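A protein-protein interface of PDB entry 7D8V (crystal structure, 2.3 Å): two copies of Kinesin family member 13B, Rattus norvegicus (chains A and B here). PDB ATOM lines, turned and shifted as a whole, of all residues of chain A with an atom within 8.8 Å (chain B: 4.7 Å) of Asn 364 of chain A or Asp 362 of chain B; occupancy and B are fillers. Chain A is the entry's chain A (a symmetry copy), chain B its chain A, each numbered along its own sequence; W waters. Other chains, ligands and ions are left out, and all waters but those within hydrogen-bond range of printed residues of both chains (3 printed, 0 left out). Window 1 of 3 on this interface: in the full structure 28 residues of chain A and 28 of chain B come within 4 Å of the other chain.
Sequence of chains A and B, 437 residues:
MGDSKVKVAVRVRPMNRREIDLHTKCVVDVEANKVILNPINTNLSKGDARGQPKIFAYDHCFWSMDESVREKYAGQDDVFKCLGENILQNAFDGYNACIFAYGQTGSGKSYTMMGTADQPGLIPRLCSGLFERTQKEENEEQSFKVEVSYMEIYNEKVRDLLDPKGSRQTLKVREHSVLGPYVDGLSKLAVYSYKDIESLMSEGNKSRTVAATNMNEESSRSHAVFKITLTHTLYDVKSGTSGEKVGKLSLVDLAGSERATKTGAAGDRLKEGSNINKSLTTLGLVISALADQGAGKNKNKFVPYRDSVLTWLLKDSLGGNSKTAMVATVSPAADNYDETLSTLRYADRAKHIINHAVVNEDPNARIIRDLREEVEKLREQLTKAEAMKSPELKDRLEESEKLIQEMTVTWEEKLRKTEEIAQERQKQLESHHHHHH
The side-chain carboxylate (OD1) of Asp 362 of chain B lies within hydrogen-bond range of the backbone NH (N) of Asn 364 of chain B (3.2 Å).
N of Asn 364 of chain A lies within hydrogen-bond range of OD1 of Asp 362 of chain A (3.2 Å).
Among the printed residues, merely in contact across the chains: Ile 368 of chain A with Ile 368 of chain B (3.3 Å), Ile 368 of chain A with Asn 364 of chain B (3.5 Å), Asn 364 of chain A with Ile 368 of chain B (3.5 Å), Asn 364 of chain A with Asp 362 of chain B (3.5 Å), Asp 362 of chain A with Asn 364 of chain B (3.5 Å), Asn 364 of chain A with Asn 364 of chain B (3.8 Å) and Leu 371 of chain A with Ile 368 of chain B (3.9 Å).
Of chain B, only Asp 362, Asn 364 and Ile 368 come within 4 Å of Asn 364 of chain A.
Asp 362 of chain B touches just one residue of chain A: Asn 364.
No residue of chain A comes within 4 Å of Pro 363 of chain B.
Of the printed residues of chain B, Ile 368 of chain A touches Asn 364 and Ile 368.
Of the printed residues of chain B, Asp 362 of chain A touches Asn 364 (3.5 Å).
Of the printed residues of chain A, Asn 364 of chain B touches Asp 362, Asn 364 and Ile 368.
Of the printed residues of chain B, Leu 371 of chain A touches Ile 368 (3.9 Å).
Printed residues of chain A within 4 Å of Ile 368 of chain B: Asn 364, Ile 368 and Leu 371.
The nearest residue of chain B that does not touch Asn 364 of chain A is Ala 365 of chain B (4.6 Å).
Of the 8 printed residues of chain B, 3 touch a printed residue of chain A.
Of the 15 printed residues of chain A, 4 touch a printed residue of chain B.
Printed residues of chain A that touch a printed residue of chain B: Asp 362, Asn 364, Ile 368 and Leu 371.
Hydrophobic or aromatic side chains of chain A within 4 Å of the printed part of chain B: Ile 368 and Leu 371.
Among the printed residues, no Asp or Glu carboxylate lies within 4 Å of a Lys or Arg side-chain nitrogen of the other chain.
Asp 362 of chain A touches Asn 364 of chain B, and with the chains exchanged Asn 364 of chain A touches Asp 362 of chain B.
Asn 364 of chain B touches its own counterpart, Asn 364 of chain A.
Asn 364 of chain A touches Ile 368 of chain B, and with the chains exchanged Ile 368 of chain A touches Asn 364 of chain B.
Ile 368 of chain B touches its own counterpart, Ile 368 of chain A.
6 positions are printed for both chains.
Of the 7 pairs that touch across the chains among the printed residues, 6 have their exchanged pair printed and touching as well.
Water W1 lies within hydrogen-bond range of the side-chain carboxylate of Asp 362 of chain B (2.5 Å), the side-chain carboxylate of Asp 362 of chain A (2.5 Å), the side-chain amide nitrogen of Asn 364 of chain B (2.9 Å) and the side-chain amide nitrogen of Asn 364 of chain A (2.9 Å).
Water W3 bridges the side-chain carboxylate (OD2) of Asp 362 of chain B (3.4 Å) and the side-chain amide nitrogen (ND2) of Asn 364 of chain A (3.5 Å).
Water W2 lies within hydrogen-bond range of the side-chain carboxylate of Asp 362 of chain A (3.4 Å) and the side-chain amide nitrogen of Asn 364 of chain B (3.5 Å).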
ATOM      1  N   THR A 241      38.223 -21.786  26.983  1.00  0.00           N
ATOM      2  CA  THR A 241      37.333 -22.002  25.852  1.00  0.00           C
ATOM      3  C   THR A 241      38.150 -22.069  24.569  1.00  0.00           C
ATOM      4  O   THR A 241      39.346 -21.792  24.555  1.00  0.00           O
ATOM      5  CB  THR A 241      36.274 -20.897  25.758  1.00  0.00           C
ATOM      6  OG1 THR A 241      36.920 -19.622  25.605  1.00  0.00           O
ATOM      7  CG2 THR A 241      35.369 -20.896  27.020  1.00  0.00           C
ATOM      8  N   SER A 242      37.495 -22.419  23.474  1.00  0.00           N
ATOM      9  CA  SER A 242      38.174 -22.494  22.191  1.00  0.00           C
ATOM     10  C   SER A 242      37.167 -22.292  21.073  1.00  0.00           C
ATOM     11  O   SER A 242      35.955 -22.394  21.273  1.00  0.00           O
ATOM     12  CB  SER A 242      38.887 -23.831  22.024  1.00  0.00           C
ATOM     13  OG  SER A 242      37.936 -24.850  21.788  1.00  0.00           O
ATOM     14  N   GLY A 243      37.693 -22.029  19.876  1.00  0.00           N
ATOM     15  CA  GLY A 243      36.842 -21.774  18.726  1.00  0.00           C
ATOM     16  C   GLY A 243      37.566 -22.079  17.436  1.00  0.00           C
ATOM     17  O   GLY A 243      38.800 -22.141  17.390  1.00  0.00           O
ATOM     18  N   GLU A 361      34.166 -17.738  11.033  1.00  0.00           N
ATOM     19  CA  GLU A 361      34.170 -18.222  12.406  1.00  0.00           C
ATOM     20  C   GLU A 361      32.730 -18.388  12.883  1.00  0.00           C
ATOM     21  O   GLU A 361      31.774 -18.034  12.185  1.00  0.00           O
ATOM     22  CB  GLU A 361      34.951 -17.278  13.328  1.00  0.00           C
ATOM     23  CG  GLU A 361      34.529 -15.825  13.274  1.00  0.00           C
ATOM     24  CD  GLU A 361      35.255 -14.993  14.309  1.00  0.00           C
ATOM     25  OE1 GLU A 361      34.593 -14.507  15.255  1.00  0.00           O
ATOM     26  OE2 GLU A 361      36.495 -14.846  14.190  1.00  0.00           O
ATOM     27  N   ASP A 362      32.580 -18.931  14.078  1.00  0.00           N
ATOM     28  CA  ASP A 362      31.248 -19.239  14.607  1.00  0.00           C
ATOM     29  C   ASP A 362      30.456 -17.962  14.878  1.00  0.00           C
ATOM     30  O   ASP A 362      30.968 -17.049  15.527  1.00  0.00           O
ATOM     31  CB  ASP A 362      31.378 -20.066  15.882  1.00  0.00           C
ATOM     32  CG  ASP A 362      30.108 -20.064  16.710  1.00  0.00           C
ATOM     33  OD1 ASP A 362      29.030 -20.376  16.159  1.00  0.00           O
ATOM     34  OD2 ASP A 362      30.196 -19.760  17.915  1.00  0.00           O
ATOM     35  N   PRO A 363      29.215 -17.858  14.403  1.00  0.00           N
ATOM     36  CA  PRO A 363      28.427 -16.625  14.637  1.00  0.00           C
ATOM     37  C   PRO A 363      27.949 -16.435  16.082  1.00  0.00           C
ATOM     38  O   PRO A 363      27.530 -15.314  16.453  1.00  0.00           O
ATOM     39  CB  PRO A 363      27.236 -16.784  13.677  1.00  0.00           C
ATOM     40  CG  PRO A 363      27.126 -18.256  13.455  1.00  0.00           C
ATOM     41  CD  PRO A 363      28.548 -18.767  13.450  1.00  0.00           C
ATOM     42  N   ASN A 364      28.001 -17.484  16.910  1.00  0.00           N
ATOM     43  CA  ASN A 364      27.443 -17.353  18.253  1.00  0.00           C
ATOM     44  C   ASN A 364      28.171 -16.283  19.059  1.00  0.00           C
ATOM     45  O   ASN A 364      27.554 -15.635  19.912  1.00  0.00           O
ATOM     46  CB  ASN A 364      27.479 -18.699  18.989  1.00  0.00           C
ATOM     47  CG  ASN A 364      26.373 -19.652  18.533  1.00  0.00           C
ATOM     48  OD1 ASN A 364      25.421 -19.248  17.852  1.00  0.00           O
ATOM     49  ND2 ASN A 364      26.514 -20.936  18.886  1.00  0.00           N
ATOM     50  N   ALA A 365      29.471 -16.070  18.797  1.00  0.00           N
ATOM     51  CA  ALA A 365      30.237 -15.124  19.610  1.00  0.00           C
ATOM     52  C   ALA A 365      29.724 -13.706  19.416  1.00  0.00           C
ATOM     53  O   ALA A 365      29.534 -12.965  20.395  1.00  0.00           O
ATOM     54  CB  ALA A 365      31.734 -15.211  19.280  1.00  0.00           C
ATOM     55  N   ARG A 366      29.478 -13.319  18.156  1.00  0.00           N
ATOM     56  CA  ARG A 366      28.886 -12.016  17.870  1.00  0.00           C
ATOM     57  C   ARG A 366      27.480 -11.913  18.458  1.00  0.00           C
ATOM     58  O   ARG A 366      27.126 -10.880  19.046  1.00  0.00           O
ATOM     59  CB  ARG A 366      28.884 -11.754  16.358  1.00  0.00           C
ATOM     60  CG  ARG A 366      28.396 -10.353  15.987  1.00  0.00           C
ATOM     61  CD  ARG A 366      29.177  -9.667  14.855  1.00  0.00           C
ATOM     62  NE  ARG A 366      29.247  -8.219  15.103  1.00  0.00           N
ATOM     63  CZ  ARG A 366      28.218  -7.368  15.029  1.00  0.00           C
ATOM     64  NH1 ARG A 366      27.005  -7.783  14.668  1.00  0.00           N
ATOM     65  NH2 ARG A 366      28.404  -6.080  15.309  1.00  0.00           N
ATOM     66  N   ILE A 367      26.671 -12.982  18.347  1.00  0.00           N
ATOM     67  CA  ILE A 367      25.331 -12.938  18.958  1.00  0.00           C
ATOM     68  C   ILE A 367      25.432 -12.697  20.470  1.00  0.00           C
ATOM     69  O   ILE A 367      24.653 -11.921  21.049  1.00  0.00           O
ATOM     70  CB  ILE A 367      24.533 -14.230  18.639  1.00  0.00           C
ATOM     71  CG1 ILE A 367      24.119 -14.290  17.166  1.00  0.00           C
ATOM     72  CG2 ILE A 367      23.281 -14.334  19.490  1.00  0.00           C
ATOM     73  CD1 ILE A 367      23.685 -15.709  16.699  1.00  0.00           C
ATOM     74  N   ILE A 368      26.403 -13.336  21.129  1.00  0.00           N
ATOM     75  CA  ILE A 368      26.550 -13.173  22.577  1.00  0.00           C
ATOM     76  C   ILE A 368      26.999 -11.749  22.924  1.00  0.00           C
ATOM     77  O   ILE A 368      26.470 -11.132  23.855  1.00  0.00           O
ATOM     78  CB  ILE A 368      27.517 -14.233  23.145  1.00  0.00           C
ATOM     79  CG1 ILE A 368      26.883 -15.623  23.053  1.00  0.00           C
ATOM     80  CG2 ILE A 368      27.902 -13.913  24.585  1.00  0.00           C
ATOM     81  CD1 ILE A 368      27.859 -16.817  23.141  1.00  0.00           C
ATOM     82  N   ARG A 369      27.992 -11.217  22.205  1.00  0.00           N
ATOM     83  CA  ARG A 369      28.429  -9.840  22.447  1.00  0.00           C
ATOM     84  C   ARG A 369      27.270  -8.862  22.287  1.00  0.00           C
ATOM     85  O   ARG A 369      27.051  -7.994  23.142  1.00  0.00           O
ATOM     86  CB  ARG A 369      29.580  -9.464  21.504  1.00  0.00           C
ATOM     87  CG  ARG A 369      30.852 -10.258  21.755  1.00  0.00           C
ATOM     88  CD  ARG A 369      32.075  -9.710  21.047  1.00  0.00           C
ATOM     89  NE  ARG A 369      31.907  -9.623  19.599  1.00  0.00           N
ATOM     90  CZ  ARG A 369      32.276 -10.575  18.751  1.00  0.00           C
ATOM     91  NH1 ARG A 369      32.831 -11.698  19.213  1.00  0.00           N
ATOM     92  NH2 ARG A 369      32.094 -10.410  17.442  1.00  0.00           N
ATOM     93  N   ASP A 370      26.500  -9.002  21.203  1.00  0.00           N
ATOM     94  CA  ASP A 370      25.379  -8.089  20.993  1.00  0.00           C
ATOM     95  C   ASP A 370      24.352  -8.220  22.110  1.00  0.00           C
ATOM     96  O   ASP A 370      23.790  -7.219  22.570  1.00  0.00           O
ATOM     97  CB  ASP A 370      24.736  -8.344  19.625  1.00  0.00           C
ATOM     98  CG  ASP A 370      25.630  -7.913  18.476  1.00  0.00           C
ATOM     99  OD1 ASP A 370      25.313  -8.235  17.308  1.00  0.00           O
ATOM    100  OD2 ASP A 370      26.661  -7.255  18.748  1.00  0.00           O
ATOM    101  N   LEU A 371      24.107  -9.445  22.578  1.00  0.00           N
ATOM    102  CA  LEU A 371      23.118  -9.634  23.631  1.00  0.00           C
ATOM    103  C   LEU A 371      23.603  -9.065  24.961  1.00  0.00           C
ATOM    104  O   LEU A 371      22.811  -8.515  25.735  1.00  0.00           O
ATOM    105  CB  LEU A 371      22.788 -11.121  23.759  1.00  0.00           C
ATOM    106  CG  LEU A 371      21.775 -11.640  22.738  1.00  0.00           C
ATOM    107  CD1 LEU A 371      21.723 -13.162  22.749  1.00  0.00           C
ATOM    108  CD2 LEU A 371      20.393 -11.061  23.035  1.00  0.00           C
ATOM    109  N   ARG A 372      24.896  -9.188  25.250  1.00  0.00           N
ATOM    110  CA  ARG A 372      25.428  -8.587  26.469  1.00  0.00           C
ATOM    111  C   ARG A 372      25.342  -7.069  26.400  1.00  0.00           C
ATOM    112  O   ARG A 372      25.008  -6.408  27.396  1.00  0.00           O
ATOM    113  CB  ARG A 372      26.874  -9.027  26.691  1.00  0.00           C
ATOM    114  CG  ARG A 372      27.049 -10.514  26.957  1.00  0.00           C
ATOM    115  CD  ARG A 372      28.138 -10.750  27.983  1.00  0.00           C
ATOM    116  NE  ARG A 372      28.079 -12.108  28.513  1.00  0.00           N
ATOM    117  CZ  ARG A 372      28.942 -13.060  28.192  1.00  0.00           C
ATOM    118  NH1 ARG A 372      29.933 -12.792  27.358  1.00  0.00           N
ATOM    119  NH2 ARG A 372      28.817 -14.272  28.708  1.00  0.00           N
ATOM    120  N   GLU B 244      28.135 -29.178  16.990  1.00  0.00           N
ATOM    121  CA  GLU B 244      28.840 -30.427  17.238  1.00  0.00           C
ATOM    122  C   GLU B 244      28.580 -30.919  18.655  1.00  0.00           C
ATOM    123  O   GLU B 244      28.571 -30.130  19.605  1.00  0.00           O
ATOM    124  CB  GLU B 244      30.347 -30.266  17.040  1.00  0.00           C
ATOM    125  CG  GLU B 244      30.748 -29.615  15.745  1.00  0.00           C
ATOM    126  CD  GLU B 244      32.244 -29.687  15.496  1.00  0.00           C
ATOM    127  OE1 GLU B 244      32.646 -30.006  14.355  1.00  0.00           O
ATOM    128  OE2 GLU B 244      33.020 -29.425  16.441  1.00  0.00           O
ATOM    129  N   ASN B 360      28.391 -33.411  25.853  1.00  0.00           N
ATOM    130  CA  ASN B 360      29.479 -32.520  25.440  1.00  0.00           C
ATOM    131  C   ASN B 360      29.080 -31.795  24.158  1.00  0.00           C
ATOM    132  O   ASN B 360      29.351 -32.249  23.046  1.00  0.00           O
ATOM    133  CB  ASN B 360      30.784 -33.291  25.266  1.00  0.00           C
ATOM    134  CG  ASN B 360      31.129 -34.132  26.485  1.00  0.00           C
ATOM    135  OD1 ASN B 360      31.339 -33.604  27.578  1.00  0.00           O
ATOM    136  ND2 ASN B 360      31.184 -35.444  26.302  1.00  0.00           N
ATOM    137  N   GLU B 361      28.443 -30.638  24.321  1.00  0.00           N
ATOM    138  CA  GLU B 361      28.135 -29.749  23.209  1.00  0.00           C
ATOM    139  C   GLU B 361      28.645 -28.348  23.530  1.00  0.00           C
ATOM    140  O   GLU B 361      29.128 -28.075  24.634  1.00  0.00           O
ATOM    141  CB  GLU B 361      26.632 -29.735  22.907  1.00  0.00           C
ATOM    142  CG  GLU B 361      25.737 -29.438  24.092  1.00  0.00           C
ATOM    143  CD  GLU B 361      24.287 -29.308  23.678  1.00  0.00           C
ATOM    144  OE1 GLU B 361      23.738 -28.186  23.772  1.00  0.00           O
ATOM    145  OE2 GLU B 361      23.702 -30.325  23.235  1.00  0.00           O
ATOM    146  N   ASP B 362      28.535 -27.460  22.558  1.00  0.00           N
ATOM    147  CA  ASP B 362      29.080 -26.107  22.705  1.00  0.00           C
ATOM    148  C   ASP B 362      28.318 -25.320  23.768  1.00  0.00           C
ATOM    149  O   ASP B 362      27.088 -25.279  23.737  1.00  0.00           O
ATOM    150  CB  ASP B 362      29.026 -25.381  21.365  1.00  0.00           C
ATOM    151  CG  ASP B 362      29.163 -23.879  21.510  1.00  0.00           C
ATOM    152  OD1 ASP B 362      30.132 -23.422  22.155  1.00  0.00           O
ATOM    153  OD2 ASP B 362      28.303 -23.158  20.967  1.00  0.00           O
ATOM    154  N   PRO B 363      29.005 -24.687  24.720  1.00  0.00           N
ATOM    155  CA  PRO B 363      28.292 -23.927  25.774  1.00  0.00           C
ATOM    156  C   PRO B 363      27.644 -22.622  25.297  1.00  0.00           C
ATOM    157  O   PRO B 363      26.792 -22.054  26.017  1.00  0.00           O
ATOM    158  CB  PRO B 363      29.395 -23.650  26.811  1.00  0.00           C
ATOM    159  CG  PRO B 363      30.667 -23.723  26.034  1.00  0.00           C
ATOM    160  CD  PRO B 363      30.447 -24.809  25.006  1.00  0.00           C
ATOM    161  N   ASN B 364      28.012 -22.130  24.108  1.00  0.00           N
ATOM    162  CA  ASN B 364      27.493 -20.831  23.690  1.00  0.00           C
ATOM    163  C   ASN B 364      25.974 -20.850  23.564  1.00  0.00           C
ATOM    164  O   ASN B 364      25.328 -19.821  23.794  1.00  0.00           O
ATOM    165  CB  ASN B 364      28.137 -20.389  22.369  1.00  0.00           C
ATOM    166  CG  ASN B 364      29.558 -19.854  22.555  1.00  0.00           C
ATOM    167  OD1 ASN B 364      29.994 -19.572  23.679  1.00  0.00           O
ATOM    168  ND2 ASN B 364      30.299 -19.741  21.445  1.00  0.00           N
ATOM    169  N   ALA B 365      25.383 -22.005  23.216  1.00  0.00           N
ATOM    170  CA  ALA B 365      23.938 -22.049  22.987  1.00  0.00           C
ATOM    171  C   ALA B 365      23.178 -21.776  24.274  1.00  0.00           C
ATOM    172  O   ALA B 365      22.217 -20.987  24.283  1.00  0.00           O
ATOM    173  CB  ALA B 365      23.524 -23.401  22.386  1.00  0.00           C
ATOM    174  N   ILE B 368      23.481 -18.138  25.153  1.00  0.00           N
ATOM    175  CA  ILE B 368      22.584 -17.305  24.349  1.00  0.00           C
ATOM    176  C   ILE B 368      21.141 -17.408  24.855  1.00  0.00           C
ATOM    177  O   ILE B 368      20.443 -16.396  24.978  1.00  0.00           O
ATOM    178  CB  ILE B 368      22.695 -17.675  22.855  1.00  0.00           C
ATOM    179  CG1 ILE B 368      24.066 -17.266  22.314  1.00  0.00           C
ATOM    180  CG2 ILE B 368      21.580 -17.027  22.041  1.00  0.00           C
ATOM    181  CD1 ILE B 368      24.510 -17.958  21.007  1.00  0.00           C
HETATM  182  O   HOH W   1      29.305 -21.532  19.394  1.00  0.00           O
HETATM  183  O   HOH W   2      32.874 -21.084  19.543  1.00  0.00           O
HETATM  184  O   HOH W   3      27.361 -24.139  17.848  1.00  0.00           O
